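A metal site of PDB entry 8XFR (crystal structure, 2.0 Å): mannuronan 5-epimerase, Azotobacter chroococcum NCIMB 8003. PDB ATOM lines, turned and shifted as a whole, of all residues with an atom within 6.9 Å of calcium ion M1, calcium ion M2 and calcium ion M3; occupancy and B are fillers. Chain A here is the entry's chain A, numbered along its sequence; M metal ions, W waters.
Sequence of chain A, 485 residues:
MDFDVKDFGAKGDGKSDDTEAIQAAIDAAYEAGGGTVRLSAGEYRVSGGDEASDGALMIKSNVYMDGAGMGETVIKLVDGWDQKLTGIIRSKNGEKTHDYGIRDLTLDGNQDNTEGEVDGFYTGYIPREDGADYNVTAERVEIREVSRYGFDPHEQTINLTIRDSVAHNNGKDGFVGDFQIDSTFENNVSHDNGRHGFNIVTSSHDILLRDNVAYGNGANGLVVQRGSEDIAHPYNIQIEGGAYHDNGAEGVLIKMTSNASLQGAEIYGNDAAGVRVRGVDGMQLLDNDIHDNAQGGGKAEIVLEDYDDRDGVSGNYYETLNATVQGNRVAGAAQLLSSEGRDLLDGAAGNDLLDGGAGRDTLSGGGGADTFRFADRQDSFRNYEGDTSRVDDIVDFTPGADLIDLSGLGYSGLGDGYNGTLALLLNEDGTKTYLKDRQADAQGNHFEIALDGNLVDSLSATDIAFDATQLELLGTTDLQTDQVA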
ATOM      1  N   ASN A 322      -2.746 -15.900   9.481  1.00  0.00           N
ATOM      2  CA  ASN A 322      -1.506 -16.651   9.709  1.00  0.00           C
ATOM      3  C   ASN A 322      -0.625 -15.982  10.750  1.00  0.00           C
ATOM      4  O   ASN A 322       0.550 -15.724  10.532  1.00  0.00           O
ATOM      5  CB  ASN A 322      -0.753 -16.815   8.396  1.00  0.00           C
ATOM      6  CG  ASN A 322      -1.542 -17.644   7.404  1.00  0.00           C
ATOM      7  OD1 ASN A 322      -2.105 -18.694   7.777  1.00  0.00           O
ATOM      8  ND2 ASN A 322      -1.690 -17.129   6.163  1.00  0.00           N
ATOM      9  N   SER A 338      -7.583 -12.835  14.512  1.00  0.00           N
ATOM     10  CA  SER A 338      -7.110 -13.306  13.210  1.00  0.00           C
ATOM     11  C   SER A 338      -8.281 -13.963  12.479  1.00  0.00           C
ATOM     12  O   SER A 338      -9.405 -14.004  12.981  1.00  0.00           O
ATOM     13  CB  SER A 338      -5.905 -14.236  13.377  1.00  0.00           C
ATOM     14  OG  SER A 338      -5.238 -14.382  12.134  1.00  0.00           O
ATOM     15  N   SER A 339      -7.991 -14.562  11.322  1.00  0.00           N
ATOM     16  CA  SER A 339      -9.028 -15.013  10.395  1.00  0.00           C
ATOM     17  C   SER A 339      -8.643 -16.403   9.881  1.00  0.00           C
ATOM     18  O   SER A 339      -7.964 -17.173  10.565  1.00  0.00           O
ATOM     19  CB  SER A 339      -9.230 -13.964   9.304  1.00  0.00           C
ATOM     20  OG  SER A 339      -9.873 -12.811   9.832  1.00  0.00           O
ATOM     21  N   GLU A 340      -9.185 -16.769   8.710  1.00  0.00           N
ATOM     22  CA  GLU A 340      -9.061 -18.110   8.136  1.00  0.00           C
ATOM     23  C   GLU A 340      -7.607 -18.645   8.195  1.00  0.00           C
ATOM     24  O   GLU A 340      -6.640 -17.896   7.994  1.00  0.00           O
ATOM     25  CB  GLU A 340      -9.545 -18.114   6.692  1.00  0.00           C
ATOM     26  CG  GLU A 340      -9.380 -19.504   6.013  1.00  0.00           C
ATOM     27  CD  GLU A 340     -10.153 -20.646   6.726  1.00  0.00           C
ATOM     28  OE1 GLU A 340     -11.354 -20.832   6.400  1.00  0.00           O
ATOM     29  OE2 GLU A 340      -9.581 -21.340   7.634  1.00  0.00           O
ATOM     30  N   GLY A 341      -7.478 -19.937   8.478  1.00  0.00           N
ATOM     31  CA  GLY A 341      -6.175 -20.557   8.664  1.00  0.00           C
ATOM     32  C   GLY A 341      -5.827 -20.700  10.147  1.00  0.00           C
ATOM     33  O   GLY A 341      -6.500 -20.168  11.033  1.00  0.00           O
ATOM     34  N   ARG A 342      -4.740 -21.418  10.404  1.00  0.00           N
ATOM     35  CA  ARG A 342      -4.360 -21.760  11.769  1.00  0.00           C
ATOM     36  C   ARG A 342      -3.598 -20.605  12.402  1.00  0.00           C
ATOM     37  O   ARG A 342      -2.561 -20.182  11.876  1.00  0.00           O
ATOM     38  CB  ARG A 342      -3.491 -23.023  11.773  1.00  0.00           C
ATOM     39  CG  ARG A 342      -2.865 -23.360  13.104  1.00  0.00           C
ATOM     40  CD  ARG A 342      -2.779 -24.897  13.259  1.00  0.00           C
ATOM     41  NE  ARG A 342      -2.103 -25.265  14.496  1.00  0.00           N
ATOM     42  CZ  ARG A 342      -2.662 -25.209  15.705  1.00  0.00           C
ATOM     43  NH1 ARG A 342      -3.912 -24.788  15.860  1.00  0.00           N
ATOM     44  NH2 ARG A 342      -1.955 -25.607  16.761  1.00  0.00           N
ATOM     45  N   ASP A 343      -4.099 -20.099  13.525  1.00  0.00           N
ATOM     46  CA  ASP A 343      -3.410 -19.090  14.310  1.00  0.00           C
ATOM     47  C   ASP A 343      -3.047 -19.665  15.664  1.00  0.00           C
ATOM     48  O   ASP A 343      -3.742 -20.527  16.184  1.00  0.00           O
ATOM     49  CB  ASP A 343      -4.329 -17.860  14.497  1.00  0.00           C
ATOM     50  CG  ASP A 343      -4.673 -17.229  13.167  1.00  0.00           C
ATOM     51  OD1 ASP A 343      -3.815 -16.471  12.657  1.00  0.00           O
ATOM     52  OD2 ASP A 343      -5.762 -17.498  12.606  1.00  0.00           O
ATOM     53  N   LEU A 345      -2.332 -17.943  19.230  1.00  0.00           N
ATOM     54  CA  LEU A 345      -2.460 -16.641  19.878  1.00  0.00           C
ATOM     55  C   LEU A 345      -2.324 -16.839  21.383  1.00  0.00           C
ATOM     56  O   LEU A 345      -3.187 -17.468  22.001  1.00  0.00           O
ATOM     57  CB  LEU A 345      -3.804 -15.986  19.516  1.00  0.00           C
ATOM     58  CG  LEU A 345      -4.072 -15.882  18.004  1.00  0.00           C
ATOM     59  CD1 LEU A 345      -5.504 -15.381  17.698  1.00  0.00           C
ATOM     60  CD2 LEU A 345      -3.062 -14.940  17.340  1.00  0.00           C
ATOM     61  N   ASP A 355      -9.335 -14.067  19.498  1.00  0.00           N
ATOM     62  CA  ASP A 355     -10.270 -14.602  18.511  1.00  0.00           C
ATOM     63  C   ASP A 355      -9.461 -15.043  17.309  1.00  0.00           C
ATOM     64  O   ASP A 355      -9.024 -14.215  16.520  1.00  0.00           O
ATOM     65  CB  ASP A 355     -11.306 -13.551  18.104  1.00  0.00           C
ATOM     66  CG  ASP A 355     -12.465 -14.152  17.272  1.00  0.00           C
ATOM     67  OD1 ASP A 355     -12.347 -15.295  16.735  1.00  0.00           O
ATOM     68  OD2 ASP A 355     -13.522 -13.473  17.171  1.00  0.00           O
ATOM     69  N   GLY A 356      -9.322 -16.349  17.138  1.00  0.00           N
ATOM     70  CA  GLY A 356      -8.644 -16.793  15.936  1.00  0.00           C
ATOM     71  C   GLY A 356      -9.493 -16.842  14.671  1.00  0.00           C
ATOM     72  O   GLY A 356      -8.950 -17.138  13.606  1.00  0.00           O
ATOM     73  N   GLY A 357     -10.794 -16.540  14.733  1.00  0.00           N
ATOM     74  CA  GLY A 357     -11.545 -16.536  13.481  1.00  0.00           C
ATOM     75  C   GLY A 357     -11.705 -17.943  12.904  1.00  0.00           C
ATOM     76  O   GLY A 357     -11.666 -18.942  13.612  1.00  0.00           O
ATOM     77  N   ALA A 358     -11.877 -18.034  11.581  1.00  0.00           N
ATOM     78  CA  ALA A 358     -12.008 -19.342  10.970  1.00  0.00           C
ATOM     79  C   ALA A 358     -10.705 -20.133  11.097  1.00  0.00           C
ATOM     80  O   ALA A 358      -9.636 -19.592  11.388  1.00  0.00           O
ATOM     81  CB  ALA A 358     -12.432 -19.212   9.509  1.00  0.00           C
ATOM     82  N   GLY A 359     -10.806 -21.457  10.925  1.00  0.00           N
ATOM     83  CA  GLY A 359      -9.649 -22.333  11.012  1.00  0.00           C
ATOM     84  C   GLY A 359      -9.391 -22.874  12.415  1.00  0.00           C
ATOM     85  O   GLY A 359      -9.972 -22.446  13.410  1.00  0.00           O
ATOM     86  N   ARG A 360      -8.455 -23.828  12.489  1.00  0.00           N
ATOM     87  CA  ARG A 360      -8.107 -24.492  13.742  1.00  0.00           C
ATOM     88  C   ARG A 360      -7.075 -23.680  14.500  1.00  0.00           C
ATOM     89  O   ARG A 360      -5.886 -23.680  14.153  1.00  0.00           O
ATOM     90  CB  ARG A 360      -7.583 -25.909  13.481  1.00  0.00           C
ATOM     91  CG  ARG A 360      -7.496 -26.721  14.765  1.00  0.00           C
ATOM     92  CD  ARG A 360      -7.041 -28.158  14.515  1.00  0.00           C
ATOM     93  NE  ARG A 360      -5.625 -28.254  14.172  1.00  0.00           N
ATOM     94  CZ  ARG A 360      -4.616 -28.240  15.038  1.00  0.00           C
ATOM     95  NH1 ARG A 360      -4.825 -28.145  16.347  1.00  0.00           N
ATOM     96  NH2 ARG A 360      -3.373 -28.318  14.575  1.00  0.00           N
ATOM     97  N   ASP A 361      -7.507 -22.985  15.551  1.00  0.00           N
ATOM     98  CA  ASP A 361      -6.627 -22.086  16.278  1.00  0.00           C
ATOM     99  C   ASP A 361      -6.336 -22.624  17.666  1.00  0.00           C
ATOM    100  O   ASP A 361      -7.157 -23.316  18.274  1.00  0.00           O
ATOM    101  CB  ASP A 361      -7.271 -20.694  16.374  1.00  0.00           C
ATOM    102  CG  ASP A 361      -7.684 -20.178  15.023  1.00  0.00           C
ATOM    103  OD1 ASP A 361      -6.837 -20.137  14.115  1.00  0.00           O
ATOM    104  OD2 ASP A 361      -8.864 -19.871  14.826  1.00  0.00           O
ATOM    105  N   THR A 362      -5.152 -22.304  18.165  1.00  0.00           N
ATOM    106  CA  THR A 362      -4.794 -22.625  19.533  1.00  0.00           C
ATOM    107  C   THR A 362      -4.606 -21.314  20.289  1.00  0.00           C
ATOM    108  O   THR A 362      -3.780 -20.490  19.893  1.00  0.00           O
ATOM    109  CB  THR A 362      -3.533 -23.485  19.570  1.00  0.00           C
ATOM    110  OG1 THR A 362      -3.811 -24.727  18.891  1.00  0.00           O
ATOM    111  CG2 THR A 362      -3.131 -23.761  20.999  1.00  0.00           C
ATOM    112  N   LEU A 363      -5.346 -21.149  21.381  1.00  0.00           N
ATOM    113  CA  LEU A 363      -5.395 -19.893  22.118  1.00  0.00           C
ATOM    114  C   LEU A 363      -5.004 -20.121  23.562  1.00  0.00           C
ATOM    115  O   LEU A 363      -5.354 -21.145  24.162  1.00  0.00           O
ATOM    116  CB  LEU A 363      -6.794 -19.262  22.078  1.00  0.00           C
ATOM    117  CG  LEU A 363      -7.530 -19.329  20.737  1.00  0.00           C
ATOM    118  CD1 LEU A 363      -9.035 -19.159  20.918  1.00  0.00           C
ATOM    119  CD2 LEU A 363      -7.018 -18.245  19.808  1.00  0.00           C
ATOM    120  N   PHE A 374     -15.719 -16.449  20.146  1.00  0.00           N
ATOM    121  CA  PHE A 374     -16.072 -17.237  18.972  1.00  0.00           C
ATOM    122  C   PHE A 374     -17.235 -16.524  18.328  1.00  0.00           C
ATOM    123  O   PHE A 374     -18.351 -16.533  18.866  1.00  0.00           O
ATOM    124  CB  PHE A 374     -16.389 -18.675  19.361  1.00  0.00           C
ATOM    125  CG  PHE A 374     -15.236 -19.345  19.995  1.00  0.00           C
ATOM    126  CD1 PHE A 374     -14.957 -19.130  21.340  1.00  0.00           C
ATOM    127  CD2 PHE A 374     -14.365 -20.103  19.237  1.00  0.00           C
ATOM    128  CE1 PHE A 374     -13.868 -19.700  21.918  1.00  0.00           C
ATOM    129  CE2 PHE A 374     -13.271 -20.671  19.807  1.00  0.00           C
ATOM    130  CZ  PHE A 374     -13.007 -20.476  21.150  1.00  0.00           C
ATOM    131  N   ALA A 375     -16.946 -15.857  17.218  1.00  0.00           N
ATOM    132  CA  ALA A 375     -17.893 -14.958  16.570  1.00  0.00           C
ATOM    133  C   ALA A 375     -18.828 -15.653  15.610  1.00  0.00           C
ATOM    134  O   ALA A 375     -19.820 -15.047  15.198  1.00  0.00           O
ATOM    135  CB  ALA A 375     -17.116 -13.877  15.811  1.00  0.00           C
ATOM    136  N   ASP A 376     -18.556 -16.906  15.233  1.00  0.00           N
ATOM    137  CA  ASP A 376     -19.255 -17.586  14.160  1.00  0.00           C
ATOM    138  C   ASP A 376     -19.224 -19.083  14.459  1.00  0.00           C
ATOM    139  O   ASP A 376     -18.196 -19.606  14.899  1.00  0.00           O
ATOM    140  CB  ASP A 376     -18.594 -17.262  12.807  1.00  0.00           C
ATOM    141  CG  ASP A 376     -19.383 -17.748  11.634  1.00  0.00           C
ATOM    142  OD1 ASP A 376     -19.596 -18.978  11.482  1.00  0.00           O
ATOM    143  OD2 ASP A 376     -19.791 -16.904  10.838  1.00  0.00           O
ATOM    144  N   ARG A 377     -20.338 -19.768  14.217  1.00  0.00           N
ATOM    145  CA  ARG A 377     -20.385 -21.203  14.490  1.00  0.00           C
ATOM    146  C   ARG A 377     -19.400 -21.984  13.631  1.00  0.00           C
ATOM    147  O   ARG A 377     -18.987 -23.089  14.015  1.00  0.00           O
ATOM    148  CB  ARG A 377     -21.810 -21.731  14.263  1.00  0.00           C
ATOM    149  CG  ARG A 377     -22.738 -21.526  15.448  1.00  0.00           C
ATOM    150  CD  ARG A 377     -24.177 -21.938  15.128  1.00  0.00           C
ATOM    151  NE  ARG A 377     -25.073 -21.524  16.208  1.00  0.00           N
ATOM    152  CZ  ARG A 377     -26.164 -22.177  16.590  1.00  0.00           C
ATOM    153  NH1 ARG A 377     -26.537 -23.304  16.008  1.00  0.00           N
ATOM    154  NH2 ARG A 377     -26.898 -21.679  17.587  1.00  0.00           N
ATOM    155  N   GLN A 378     -18.996 -21.439  12.485  1.00  0.00           N
ATOM    156  CA  GLN A 378     -18.050 -22.092  11.616  1.00  0.00           C
ATOM    157  C   GLN A 378     -16.599 -21.737  11.956  1.00  0.00           C
ATOM    158  O   GLN A 378     -15.685 -22.087  11.202  1.00  0.00           O
ATOM    159  CB  GLN A 378     -18.352 -21.729  10.148  1.00  0.00           C
ATOM    160  CG  GLN A 378     -19.699 -22.235   9.602  1.00  0.00           C
ATOM    161  CD  GLN A 378     -19.963 -23.723   9.845  1.00  0.00           C
ATOM    162  OE1 GLN A 378     -19.213 -24.600   9.346  1.00  0.00           O
ATOM    163  NE2 GLN A 378     -21.025 -24.027  10.609  1.00  0.00           N
ATOM    164  N   ASP A 379     -16.362 -21.062  13.069  1.00  0.00           N
ATOM    165  CA  ASP A 379     -14.994 -20.727  13.423  1.00  0.00           C
ATOM    166  C   ASP A 379     -14.308 -21.824  14.224  1.00  0.00           C
ATOM    167  O   ASP A 379     -13.079 -21.788  14.355  1.00  0.00           O
ATOM    168  CB  ASP A 379     -14.981 -19.425  14.210  1.00  0.00           C
ATOM    169  CG  ASP A 379     -15.262 -18.201  13.309  1.00  0.00           C
ATOM    170  OD1 ASP A 379     -15.315 -18.368  12.059  1.00  0.00           O
ATOM    171  OD2 ASP A 379     -15.424 -17.107  13.844  1.00  0.00           O
ATOM    172  N   SER A 380     -15.068 -22.799  14.715  1.00  0.00           N
ATOM    173  CA  SER A 380     -14.531 -23.916  15.501  1.00  0.00           C
ATOM    174  C   SER A 380     -15.562 -25.020  15.394  1.00  0.00           C
ATOM    175  O   SER A 380     -16.654 -24.868  15.944  1.00  0.00           O
ATOM    176  CB  SER A 380     -14.292 -23.500  16.958  1.00  0.00           C
ATOM    177  OG  SER A 380     -13.565 -24.479  17.689  1.00  0.00           O
ATOM    178  N   PHE A 381     -15.252 -26.094  14.657  1.00  0.00           N
ATOM    179  CA  PHE A 381     -16.274 -27.071  14.281  1.00  0.00           C
ATOM    180  C   PHE A 381     -15.656 -28.410  13.890  1.00  0.00           C
ATOM    181  O   PHE A 381     -14.493 -28.510  13.493  1.00  0.00           O
ATOM    182  CB  PHE A 381     -17.148 -26.539  13.133  1.00  0.00           C
ATOM    183  CG  PHE A 381     -16.477 -26.576  11.782  1.00  0.00           C
ATOM    184  CD1 PHE A 381     -15.647 -25.532  11.375  1.00  0.00           C
ATOM    185  CD2 PHE A 381     -16.677 -27.642  10.913  1.00  0.00           C
ATOM    186  CE1 PHE A 381     -15.029 -25.563  10.136  1.00  0.00           C
ATOM    187  CE2 PHE A 381     -16.055 -27.671   9.666  1.00  0.00           C
ATOM    188  CZ  PHE A 381     -15.227 -26.632   9.280  1.00  0.00           C
ATOM    189  N   ARG A 390     -10.128 -28.300  12.473  1.00  0.00           N
ATOM    190  CA  ARG A 390     -10.966 -27.110  12.511  1.00  0.00           C
ATOM    191  C   ARG A 390     -11.617 -26.905  13.885  1.00  0.00           C
ATOM    192  O   ARG A 390     -12.384 -25.963  14.037  1.00  0.00           O
ATOM    193  CB  ARG A 390     -12.050 -27.106  11.420  1.00  0.00           C
ATOM    194  CG  ARG A 390     -11.593 -27.363   9.959  1.00  0.00           C
ATOM    195  CD  ARG A 390     -10.254 -26.757   9.544  1.00  0.00           C
ATOM    196  NE  ARG A 390      -9.096 -27.626   9.730  1.00  0.00           N
ATOM    197  CZ  ARG A 390      -8.853 -28.723   9.017  1.00  0.00           C
ATOM    198  NH1 ARG A 390      -9.741 -29.211   8.166  1.00  0.00           N
ATOM    199  NH2 ARG A 390      -7.688 -29.350   9.174  1.00  0.00           N
ATOM    200  N   VAL A 391     -11.314 -27.720  14.885  1.00  0.00           N
ATOM    201  CA  VAL A 391     -11.749 -27.443  16.256  1.00  0.00           C
ATOM    202  C   VAL A 391     -10.660 -26.674  17.005  1.00  0.00           C
ATOM    203  O   VAL A 391      -9.542 -27.178  17.181  1.00  0.00           O
ATOM    204  CB  VAL A 391     -12.151 -28.725  16.996  1.00  0.00           C
ATOM    205  CG1 VAL A 391     -12.470 -28.415  18.461  1.00  0.00           C
ATOM    206  CG2 VAL A 391     -13.378 -29.338  16.312  1.00  0.00           C
ATOM    207  N   ASP A 392     -10.992 -25.470  17.466  1.00  0.00           N
ATOM    208  CA  ASP A 392     -10.075 -24.679  18.291  1.00  0.00           C
ATOM    209  C   ASP A 392      -9.817 -25.358  19.628  1.00  0.00           C
ATOM    210  O   ASP A 392     -10.694 -26.022  20.182  1.00  0.00           O
ATOM    211  CB  ASP A 392     -10.669 -23.299  18.597  1.00  0.00           C
ATOM    212  CG  ASP A 392     -10.691 -22.368  17.402  1.00  0.00           C
ATOM    213  OD1 ASP A 392     -10.289 -22.790  16.294  1.00  0.00           O
ATOM    214  OD2 ASP A 392     -11.076 -21.201  17.605  1.00  0.00           O
HETATM  215 CA    CA M   1      -7.761 -18.755  12.366  1.00  0.00          CA
HETATM  216 CA    CA M   2     -10.998 -20.943  14.912  1.00  0.00          CA
HETATM  217 CA    CA M   3     -16.457 -16.182  11.158  1.00  0.00          CA
HETATM  218  O   HOH W   1     -15.171 -16.789   9.262  1.00  0.00           O
HETATM  219  O   HOH W   2     -12.321 -19.380  16.320  1.00  0.00           O
HETATM  220  O   HOH W   3     -15.394 -14.544  12.494  1.00  0.00           O
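The side-chain hydroxyl (OG) of Ser 380 lies within hydrogen-bond range of the backbone NH (N) of Asp 392, at 2.8 Å.
The backbone NH of Ala 358 sits close to the side-chain carboxylate of Asp 379 (3.5 Å).
N of Gly 357 lies within hydrogen-bond range of OD1 of Asp 355, at 2.8 Å.
N of Asp 376 sits close to OD2 of Asp 379 (3.4 Å).
The backbone carbonyl oxygen of Asp 343 lies within hydrogen-bond range of the backbone NH of Thr 362 (3.0 Å).
The side-chain carboxylate (OD1) of Asp 343 is in hydrogen-bond range of the backbone NH (N) of Asn 322, at 3.4 Å.
OD1 of Asp 376 lies within hydrogen-bond range of N of Gln 378 (2.7 Å).
The side-chain carboxylate (OD1) of Asp 343 lies within hydrogen-bond range of the side-chain hydroxyl (OG) of Ser 338 (2.6 Å).
Calcium ion M1 is bound by O of Ala 358 (2.3 Å), O of Gly 341 (2.3 Å), O of Gly 356 (2.4 Å), OD2 of Asp 343 (2.4 Å), O of Ser 339 (2.4 Å) and OD1 of Asp 361 (2.4 Å).
Slightly farther from calcium ion M1 lies OD2 of Asp 361 (2.9 Å).
Residues that only touch calcium ion M3: Asp 376 (2.9 Å).
Of the 28 residues printed, 2 come within 4 Å of calcium ion M3.
Water W3 is bound to calcium ion M3.
Water W1 binds calcium ion M3 (2.4 Å).
OD1 of Asp 379 binds calcium ion M3 (2.6 Å).
Calcium ion M3 has three donor atoms within binding distance.
Slightly farther from calcium ion M3 lies OD2 of Asp 379 (3.0 Å).
Within 4 Å of calcium ion M2: Gly 357, Ala 358, Gly 359, Asp 361, Asp 379 and Asp 392.
The nearest printed residue that does not touch calcium ion M2 is Gly 356 (4.4 Å).
Of the 28 residues printed, 6 come within 4 Å of calcium ion M1.
Along chain A the residues within 4 Å of calcium ion M1 span positions 339 to 361.
The nearest printed residue that does not touch calcium ion M1 is Gly 357 (4.1 Å).
Calcium ion M2 is bound by O of Asp 379 (2.3 Å).
O of Gly 359 binds calcium ion M2 (2.4 Å).
Calcium ion M2 is bound by OD2 of Asp 361, 2.4 Å away.
The side-chain carboxylate (OD1) of Asp 392 is bound to calcium ion M2 (2.4 Å).
Calcium ion M2 is bound by O of Gly 357 (2.5 Å).
Calcium ion M2 is bound by water W2 (2.5 Å).
Calcium ion M2 is bound by the side-chain carboxylate (OD2) of Asp 392.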
